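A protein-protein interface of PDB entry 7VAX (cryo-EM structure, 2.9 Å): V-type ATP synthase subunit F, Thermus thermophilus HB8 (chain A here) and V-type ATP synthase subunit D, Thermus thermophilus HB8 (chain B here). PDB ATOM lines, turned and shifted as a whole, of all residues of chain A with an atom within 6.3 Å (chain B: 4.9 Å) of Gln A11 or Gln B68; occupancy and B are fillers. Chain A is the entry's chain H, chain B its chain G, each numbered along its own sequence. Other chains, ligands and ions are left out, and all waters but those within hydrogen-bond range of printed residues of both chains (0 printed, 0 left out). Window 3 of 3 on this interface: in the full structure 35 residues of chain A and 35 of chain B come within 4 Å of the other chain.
Among the printed residues, merely in contact across the chains: Glu A8 with Leu B64, Leu A15 with Ala B80 and Glu A8 with Leu B65.
Printed residues of chain B that touch a printed residue of chain A: Leu B64, Leu B65, Gln B68 and Ala B80.
Of the 12 printed residues of chain A, 4 touch a printed residue of chain B.
Printed residues of chain A that touch a printed residue of chain B: Glu A8, Gln A11, Arg A14 and Leu A15.
Among the printed residues, 6 pairs touch across the chains.
Among the printed residues, no Asp or Glu carboxylate lies within 4 Å of a Lys or Arg side-chain nitrogen of the other chain.
The side-chain amide nitrogen (NE2) of Gln B68 sits at hydrogen-bond distance from the side-chain amide oxygen (OE1) of Gln A11, 3.3 Å away.
OE1 of Gln B68 sits close to OE2 of Glu A8.
The backbone carbonyl oxygen (O) of Arg A14 lies close to the backbone carbonyl oxygen (O) of Ala B80, 3.4 Å away.
Of the printed residues of chain B, Gln A11 touches Gln B68 (3.3 Å).
Printed residues of chain B within 4 Å of Leu A15: Ala B80.
Ala A16 touches none of the printed residues of chain B.
Of the printed residues of chain A, Leu B65 touches Glu A8 (3.8 Å).
Of chain A, only Glu A8 and Gln A11 come within 4 Å of Gln B68.
Phe B70 touches none of the printed residues of chain A.
Printed residues of chain A within 4 Å of Ala B80: Arg A14 and Leu A15.
The nearest residue of chain B that does not touch Gln A11 is Ala B80 (4.1 Å).
The nearest printed residue of chain A that does not touch Leu B65 is Asp A6 (8.5 Å).
The backbone NH (N) of Glu A8 lies close to the side-chain carboxylate (OD2) of Asp A6 (3.5 Å).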
ATOM      1  N   ASP A   6     -22.982  -5.357 -12.131  1.00  0.00           N
ATOM      2  CA  ASP A   6     -22.486  -6.505 -12.877  1.00  0.00           C
ATOM      3  C   ASP A   6     -21.710  -5.988 -14.083  1.00  0.00           C
ATOM      4  O   ASP A   6     -21.838  -4.812 -14.444  1.00  0.00           O
ATOM      5  CB  ASP A   6     -23.639  -7.429 -13.314  1.00  0.00           C
ATOM      6  CG  ASP A   6     -24.373  -6.917 -14.537  1.00  0.00           C
ATOM      7  OD1 ASP A   6     -24.622  -5.699 -14.622  1.00  0.00           O
ATOM      8  OD2 ASP A   6     -24.692  -7.737 -15.422  1.00  0.00           O
ATOM      9  N   PRO A   7     -20.886  -6.833 -14.716  1.00  0.00           N
ATOM     10  CA  PRO A   7     -20.077  -6.344 -15.847  1.00  0.00           C
ATOM     11  C   PRO A   7     -20.899  -5.777 -16.992  1.00  0.00           C
ATOM     12  O   PRO A   7     -20.428  -4.863 -17.677  1.00  0.00           O
ATOM     13  CB  PRO A   7     -19.289  -7.590 -16.282  1.00  0.00           C
ATOM     14  CG  PRO A   7     -20.030  -8.746 -15.697  1.00  0.00           C
ATOM     15  CD  PRO A   7     -20.586  -8.242 -14.410  1.00  0.00           C
ATOM     16  N   GLU A   8     -22.110  -6.289 -17.224  1.00  0.00           N
ATOM     17  CA  GLU A   8     -22.956  -5.730 -18.274  1.00  0.00           C
ATOM     18  C   GLU A   8     -23.319  -4.281 -17.970  1.00  0.00           C
ATOM     19  O   GLU A   8     -23.124  -3.388 -18.805  1.00  0.00           O
ATOM     20  CB  GLU A   8     -24.217  -6.581 -18.435  1.00  0.00           C
ATOM     21  CG  GLU A   8     -25.130  -6.148 -19.571  1.00  0.00           C
ATOM     22  CD  GLU A   8     -24.620  -6.580 -20.932  1.00  0.00           C
ATOM     23  OE1 GLU A   8     -23.635  -7.346 -20.986  1.00  0.00           O
ATOM     24  OE2 GLU A   8     -25.208  -6.157 -21.949  1.00  0.00           O
ATOM     25  N   THR A   9     -23.836  -4.025 -16.766  1.00  0.00           N
ATOM     26  CA  THR A   9     -24.179  -2.660 -16.384  1.00  0.00           C
ATOM     27  C   THR A   9     -22.938  -1.789 -16.244  1.00  0.00           C
ATOM     28  O   THR A   9     -22.987  -0.592 -16.546  1.00  0.00           O
ATOM     29  CB  THR A   9     -24.977  -2.656 -15.079  1.00  0.00           C
ATOM     30  OG1 THR A   9     -26.069  -3.579 -15.184  1.00  0.00           O
ATOM     31  CG2 THR A   9     -25.524  -1.272 -14.789  1.00  0.00           C
ATOM     32  N   ALA A  10     -21.823  -2.364 -15.788  1.00  0.00           N
ATOM     33  CA  ALA A  10     -20.582  -1.601 -15.703  1.00  0.00           C
ATOM     34  C   ALA A  10     -20.142  -1.125 -17.082  1.00  0.00           C
ATOM     35  O   ALA A  10     -19.781   0.042 -17.264  1.00  0.00           O
ATOM     36  CB  ALA A  10     -19.491  -2.443 -15.044  1.00  0.00           C
ATOM     37  N   GLN A  11     -20.184  -2.019 -18.073  1.00  0.00           N
ATOM     38  CA  GLN A  11     -19.848  -1.633 -19.440  1.00  0.00           C
ATOM     39  C   GLN A  11     -20.833  -0.605 -19.979  1.00  0.00           C
ATOM     40  O   GLN A  11     -20.437   0.351 -20.656  1.00  0.00           O
ATOM     41  CB  GLN A  11     -19.821  -2.867 -20.342  1.00  0.00           C
ATOM     42  CG  GLN A  11     -18.530  -3.665 -20.276  1.00  0.00           C
ATOM     43  CD  GLN A  11     -18.487  -4.784 -21.298  1.00  0.00           C
ATOM     44  OE1 GLN A  11     -19.206  -4.755 -22.297  1.00  0.00           O
ATOM     45  NE2 GLN A  11     -17.640  -5.777 -21.054  1.00  0.00           N
ATOM     46  N   GLY A  12     -22.124  -0.787 -19.691  1.00  0.00           N
ATOM     47  CA  GLY A  12     -23.117   0.157 -20.178  1.00  0.00           C
ATOM     48  C   GLY A  12     -22.921   1.552 -19.619  1.00  0.00           C
ATOM     49  O   GLY A  12     -23.035   2.547 -20.339  1.00  0.00           O
ATOM     50  N   PHE A  13     -22.625   1.644 -18.321  1.00  0.00           N
ATOM     51  CA  PHE A  13     -22.369   2.943 -17.711  1.00  0.00           C
ATOM     52  C   PHE A  13     -21.043   3.526 -18.177  1.00  0.00           C
ATOM     53  O   PHE A  13     -20.916   4.751 -18.300  1.00  0.00           O
ATOM     54  CB  PHE A  13     -22.397   2.824 -16.188  1.00  0.00           C
ATOM     55  CG  PHE A  13     -23.751   3.071 -15.591  1.00  0.00           C
ATOM     56  CD1 PHE A  13     -24.672   2.046 -15.485  1.00  0.00           C
ATOM     57  CD2 PHE A  13     -24.104   4.332 -15.144  1.00  0.00           C
ATOM     58  CE1 PHE A  13     -25.919   2.270 -14.936  1.00  0.00           C
ATOM     59  CE2 PHE A  13     -25.351   4.563 -14.595  1.00  0.00           C
ATOM     60  CZ  PHE A  13     -26.259   3.531 -14.492  1.00  0.00           C
ATOM     61  N   ARG A  14     -20.044   2.675 -18.429  1.00  0.00           N
ATOM     62  CA  ARG A  14     -18.798   3.147 -19.021  1.00  0.00           C
ATOM     63  C   ARG A  14     -19.053   3.771 -20.386  1.00  0.00           C
ATOM     64  O   ARG A  14     -18.439   4.785 -20.740  1.00  0.00           O
ATOM     65  CB  ARG A  14     -17.807   1.988 -19.130  1.00  0.00           C
ATOM     66  CG  ARG A  14     -16.449   2.363 -19.694  1.00  0.00           C
ATOM     67  CD  ARG A  14     -15.659   3.214 -18.717  1.00  0.00           C
ATOM     68  NE  ARG A  14     -15.715   4.629 -19.066  1.00  0.00           N
ATOM     69  CZ  ARG A  14     -15.025   5.579 -18.452  1.00  0.00           C
ATOM     70  NH1 ARG A  14     -14.213   5.302 -17.445  1.00  0.00           N
ATOM     71  NH2 ARG A  14     -15.150   6.837 -18.861  1.00  0.00           N
ATOM     72  N   LEU A  15     -19.956   3.176 -21.166  1.00  0.00           N
ATOM     73  CA  LEU A  15     -20.343   3.768 -22.441  1.00  0.00           C
ATOM     74  C   LEU A  15     -21.042   5.107 -22.237  1.00  0.00           C
ATOM     75  O   LEU A  15     -20.787   6.068 -22.974  1.00  0.00           O
ATOM     76  CB  LEU A  15     -21.243   2.800 -23.211  1.00  0.00           C
ATOM     77  CG  LEU A  15     -22.055   3.376 -24.371  1.00  0.00           C
ATOM     78  CD1 LEU A  15     -21.136   3.897 -25.467  1.00  0.00           C
ATOM     79  CD2 LEU A  15     -23.018   2.335 -24.923  1.00  0.00           C
ATOM     80  N   ALA A  16     -21.926   5.192 -21.240  1.00  0.00           N
ATOM     81  CA  ALA A  16     -22.650   6.436 -20.996  1.00  0.00           C
ATOM     82  C   ALA A  16     -21.744   7.518 -20.425  1.00  0.00           C
ATOM     83  O   ALA A  16     -22.043   8.710 -20.561  1.00  0.00           O
ATOM     84  CB  ALA A  16     -23.826   6.188 -20.055  1.00  0.00           C
ATOM     85  N   GLY A  20     -17.299   2.057 -14.193  1.00  0.00           N
ATOM     86  CA  GLY A  20     -17.601   0.933 -13.326  1.00  0.00           C
ATOM     87  C   GLY A  20     -16.358   0.116 -13.045  1.00  0.00           C
ATOM     88  O   GLY A  20     -15.415   0.132 -13.841  1.00  0.00           O
ATOM     89  N   LEU B  64     -28.834  -2.009 -25.001  1.00  0.00           N
ATOM     90  CA  LEU B  64     -27.477  -2.539 -24.885  1.00  0.00           C
ATOM     91  C   LEU B  64     -27.384  -3.954 -25.440  1.00  0.00           C
ATOM     92  O   LEU B  64     -26.419  -4.293 -26.136  1.00  0.00           O
ATOM     93  CB  LEU B  64     -27.014  -2.511 -23.430  1.00  0.00           C
ATOM     94  CG  LEU B  64     -25.558  -2.944 -23.233  1.00  0.00           C
ATOM     95  CD1 LEU B  64     -24.627  -2.084 -24.074  1.00  0.00           C
ATOM     96  CD2 LEU B  64     -25.151  -2.916 -21.767  1.00  0.00           C
ATOM     97  N   LEU B  65     -28.370  -4.801 -25.130  1.00  0.00           N
ATOM     98  CA  LEU B  65     -28.360  -6.162 -25.660  1.00  0.00           C
ATOM     99  C   LEU B  65     -28.477  -6.163 -27.178  1.00  0.00           C
ATOM    100  O   LEU B  65     -27.792  -6.933 -27.862  1.00  0.00           O
ATOM    101  CB  LEU B  65     -29.484  -6.984 -25.031  1.00  0.00           C
ATOM    102  CG  LEU B  65     -29.369  -7.235 -23.526  1.00  0.00           C
ATOM    103  CD1 LEU B  65     -30.644  -7.866 -22.988  1.00  0.00           C
ATOM    104  CD2 LEU B  65     -28.162  -8.108 -23.216  1.00  0.00           C
ATOM    105  N   LEU B  66     -29.336  -5.299 -27.727  1.00  0.00           N
ATOM    106  CA  LEU B  66     -29.466  -5.217 -29.178  1.00  0.00           C
ATOM    107  C   LEU B  66     -28.162  -4.754 -29.817  1.00  0.00           C
ATOM    108  O   LEU B  66     -27.757  -5.271 -30.867  1.00  0.00           O
ATOM    109  CB  LEU B  66     -30.623  -4.283 -29.543  1.00  0.00           C
ATOM    110  CG  LEU B  66     -31.095  -4.206 -30.998  1.00  0.00           C
ATOM    111  CD1 LEU B  66     -32.572  -3.850 -31.044  1.00  0.00           C
ATOM    112  CD2 LEU B  66     -30.295  -3.191 -31.796  1.00  0.00           C
ATOM    113  N   ALA B  67     -27.489  -3.779 -29.201  1.00  0.00           N
ATOM    114  CA  ALA B  67     -26.221  -3.295 -29.738  1.00  0.00           C
ATOM    115  C   ALA B  67     -25.143  -4.370 -29.674  1.00  0.00           C
ATOM    116  O   ALA B  67     -24.348  -4.513 -30.609  1.00  0.00           O
ATOM    117  CB  ALA B  67     -25.776  -2.043 -28.985  1.00  0.00           C
ATOM    118  N   GLN B  68     -25.096  -5.133 -28.579  1.00  0.00           N
ATOM    119  CA  GLN B  68     -24.101  -6.190 -28.450  1.00  0.00           C
ATOM    120  C   GLN B  68     -24.415  -7.402 -29.315  1.00  0.00           C
ATOM    121  O   GLN B  68     -23.514  -8.204 -29.584  1.00  0.00           O
ATOM    122  CB  GLN B  68     -23.970  -6.623 -26.989  1.00  0.00           C
ATOM    123  CG  GLN B  68     -22.919  -5.850 -26.209  1.00  0.00           C
ATOM    124  CD  GLN B  68     -22.895  -6.220 -24.740  1.00  0.00           C
ATOM    125  OE1 GLN B  68     -23.734  -6.986 -24.267  1.00  0.00           O
ATOM    126  NE2 GLN B  68     -21.928  -5.678 -24.009  1.00  0.00           N
ATOM    127  N   ALA B  69     -25.668  -7.563 -29.744  1.00  0.00           N
ATOM    128  CA  ALA B  69     -25.993  -8.644 -30.667  1.00  0.00           C
ATOM    129  C   ALA B  69     -25.709  -8.244 -32.110  1.00  0.00           C
ATOM    130  O   ALA B  69     -25.098  -9.008 -32.865  1.00  0.00           O
ATOM    131  CB  ALA B  69     -27.456  -9.057 -30.500  1.00  0.00           C
ATOM    132  N   PHE B  70     -26.146  -7.048 -32.511  1.00  0.00           N
ATOM    133  CA  PHE B  70     -25.903  -6.589 -33.875  1.00  0.00           C
ATOM    134  C   PHE B  70     -24.429  -6.265 -34.093  1.00  0.00           C
ATOM    135  O   PHE B  70     -23.836  -6.668 -35.101  1.00  0.00           O
ATOM    136  CB  PHE B  70     -26.777  -5.373 -34.185  1.00  0.00           C
ATOM    137  CG  PHE B  70     -28.183  -5.724 -34.582  1.00  0.00           C
ATOM    138  CD1 PHE B  70     -29.060  -6.278 -33.666  1.00  0.00           C
ATOM    139  CD2 PHE B  70     -28.626  -5.501 -35.876  1.00  0.00           C
ATOM    140  CE1 PHE B  70     -30.353  -6.602 -34.030  1.00  0.00           C
ATOM    141  CE2 PHE B  70     -29.918  -5.821 -36.246  1.00  0.00           C
ATOM    142  CZ  PHE B  70     -30.782  -6.373 -35.322  1.00  0.00           C
ATOM    143  N   ASP B  71     -23.822  -5.538 -33.160  1.00  0.00           N
ATOM    144  CA  ASP B  71     -22.413  -5.185 -33.230  1.00  0.00           C
ATOM    145  C   ASP B  71     -21.624  -6.001 -32.215  1.00  0.00           C
ATOM    146  O   ASP B  71     -22.152  -6.409 -31.178  1.00  0.00           O
ATOM    147  CB  ASP B  71     -22.206  -3.689 -32.973  1.00  0.00           C
ATOM    148  CG  ASP B  71     -22.912  -2.818 -33.994  1.00  0.00           C
ATOM    149  OD1 ASP B  71     -22.989  -3.227 -35.172  1.00  0.00           O
ATOM    150  OD2 ASP B  71     -23.387  -1.725 -33.621  1.00  0.00           O
ATOM    151  N   GLY B  72     -20.352  -6.236 -32.527  1.00  0.00           N
ATOM    152  CA  GLY B  72     -19.498  -7.047 -31.691  1.00  0.00           C
ATOM    153  C   GLY B  72     -19.303  -6.467 -30.305  1.00  0.00           C
ATOM    154  O   GLY B  72     -19.208  -5.251 -30.122  1.00  0.00           O
ATOM    155  N   PRO B  73     -19.262  -7.335 -29.293  1.00  0.00           N
ATOM    156  CA  PRO B  73     -19.003  -6.849 -27.927  1.00  0.00           C
ATOM    157  C   PRO B  73     -17.659  -6.155 -27.779  1.00  0.00           C
ATOM    158  O   PRO B  73     -17.546  -5.207 -26.991  1.00  0.00           O
ATOM    159  CB  PRO B  73     -19.073  -8.128 -27.081  1.00  0.00           C
ATOM    160  CG  PRO B  73     -19.881  -9.086 -27.897  1.00  0.00           C
ATOM    161  CD  PRO B  73     -19.554  -8.777 -29.325  1.00  0.00           C
ATOM    162  N   VAL B  76     -17.837  -2.646 -28.965  1.00  0.00           N
ATOM    163  CA  VAL B  76     -18.633  -1.907 -27.988  1.00  0.00           C
ATOM    164  C   VAL B  76     -17.772  -1.508 -26.795  1.00  0.00           C
ATOM    165  O   VAL B  76     -17.835  -0.368 -26.317  1.00  0.00           O
ATOM    166  CB  VAL B  76     -19.854  -2.738 -27.556  1.00  0.00           C
ATOM    167  CG1 VAL B  76     -20.507  -2.129 -26.325  1.00  0.00           C
ATOM    168  CG2 VAL B  76     -20.856  -2.840 -28.696  1.00  0.00           C
ATOM    169  N   ALA B  77     -16.954  -2.439 -26.299  1.00  0.00           N
ATOM    170  CA  ALA B  77     -16.048  -2.118 -25.200  1.00  0.00           C
ATOM    171  C   ALA B  77     -15.034  -1.059 -25.615  1.00  0.00           C
ATOM    172  O   ALA B  77     -14.712  -0.154 -24.836  1.00  0.00           O
ATOM    173  CB  ALA B  77     -15.340  -3.383 -24.717  1.00  0.00           C
ATOM    174  N   ALA B  80     -16.779   2.240 -25.578  1.00  0.00           N
ATOM    175  CA  ALA B  80     -16.979   2.672 -24.198  1.00  0.00           C
ATOM    176  C   ALA B  80     -15.679   3.151 -23.566  1.00  0.00           C
ATOM    177  O   ALA B  80     -15.701   3.983 -22.652  1.00  0.00           O
ATOM    178  CB  ALA B  80     -17.581   1.535 -23.374  1.00  0.00           C
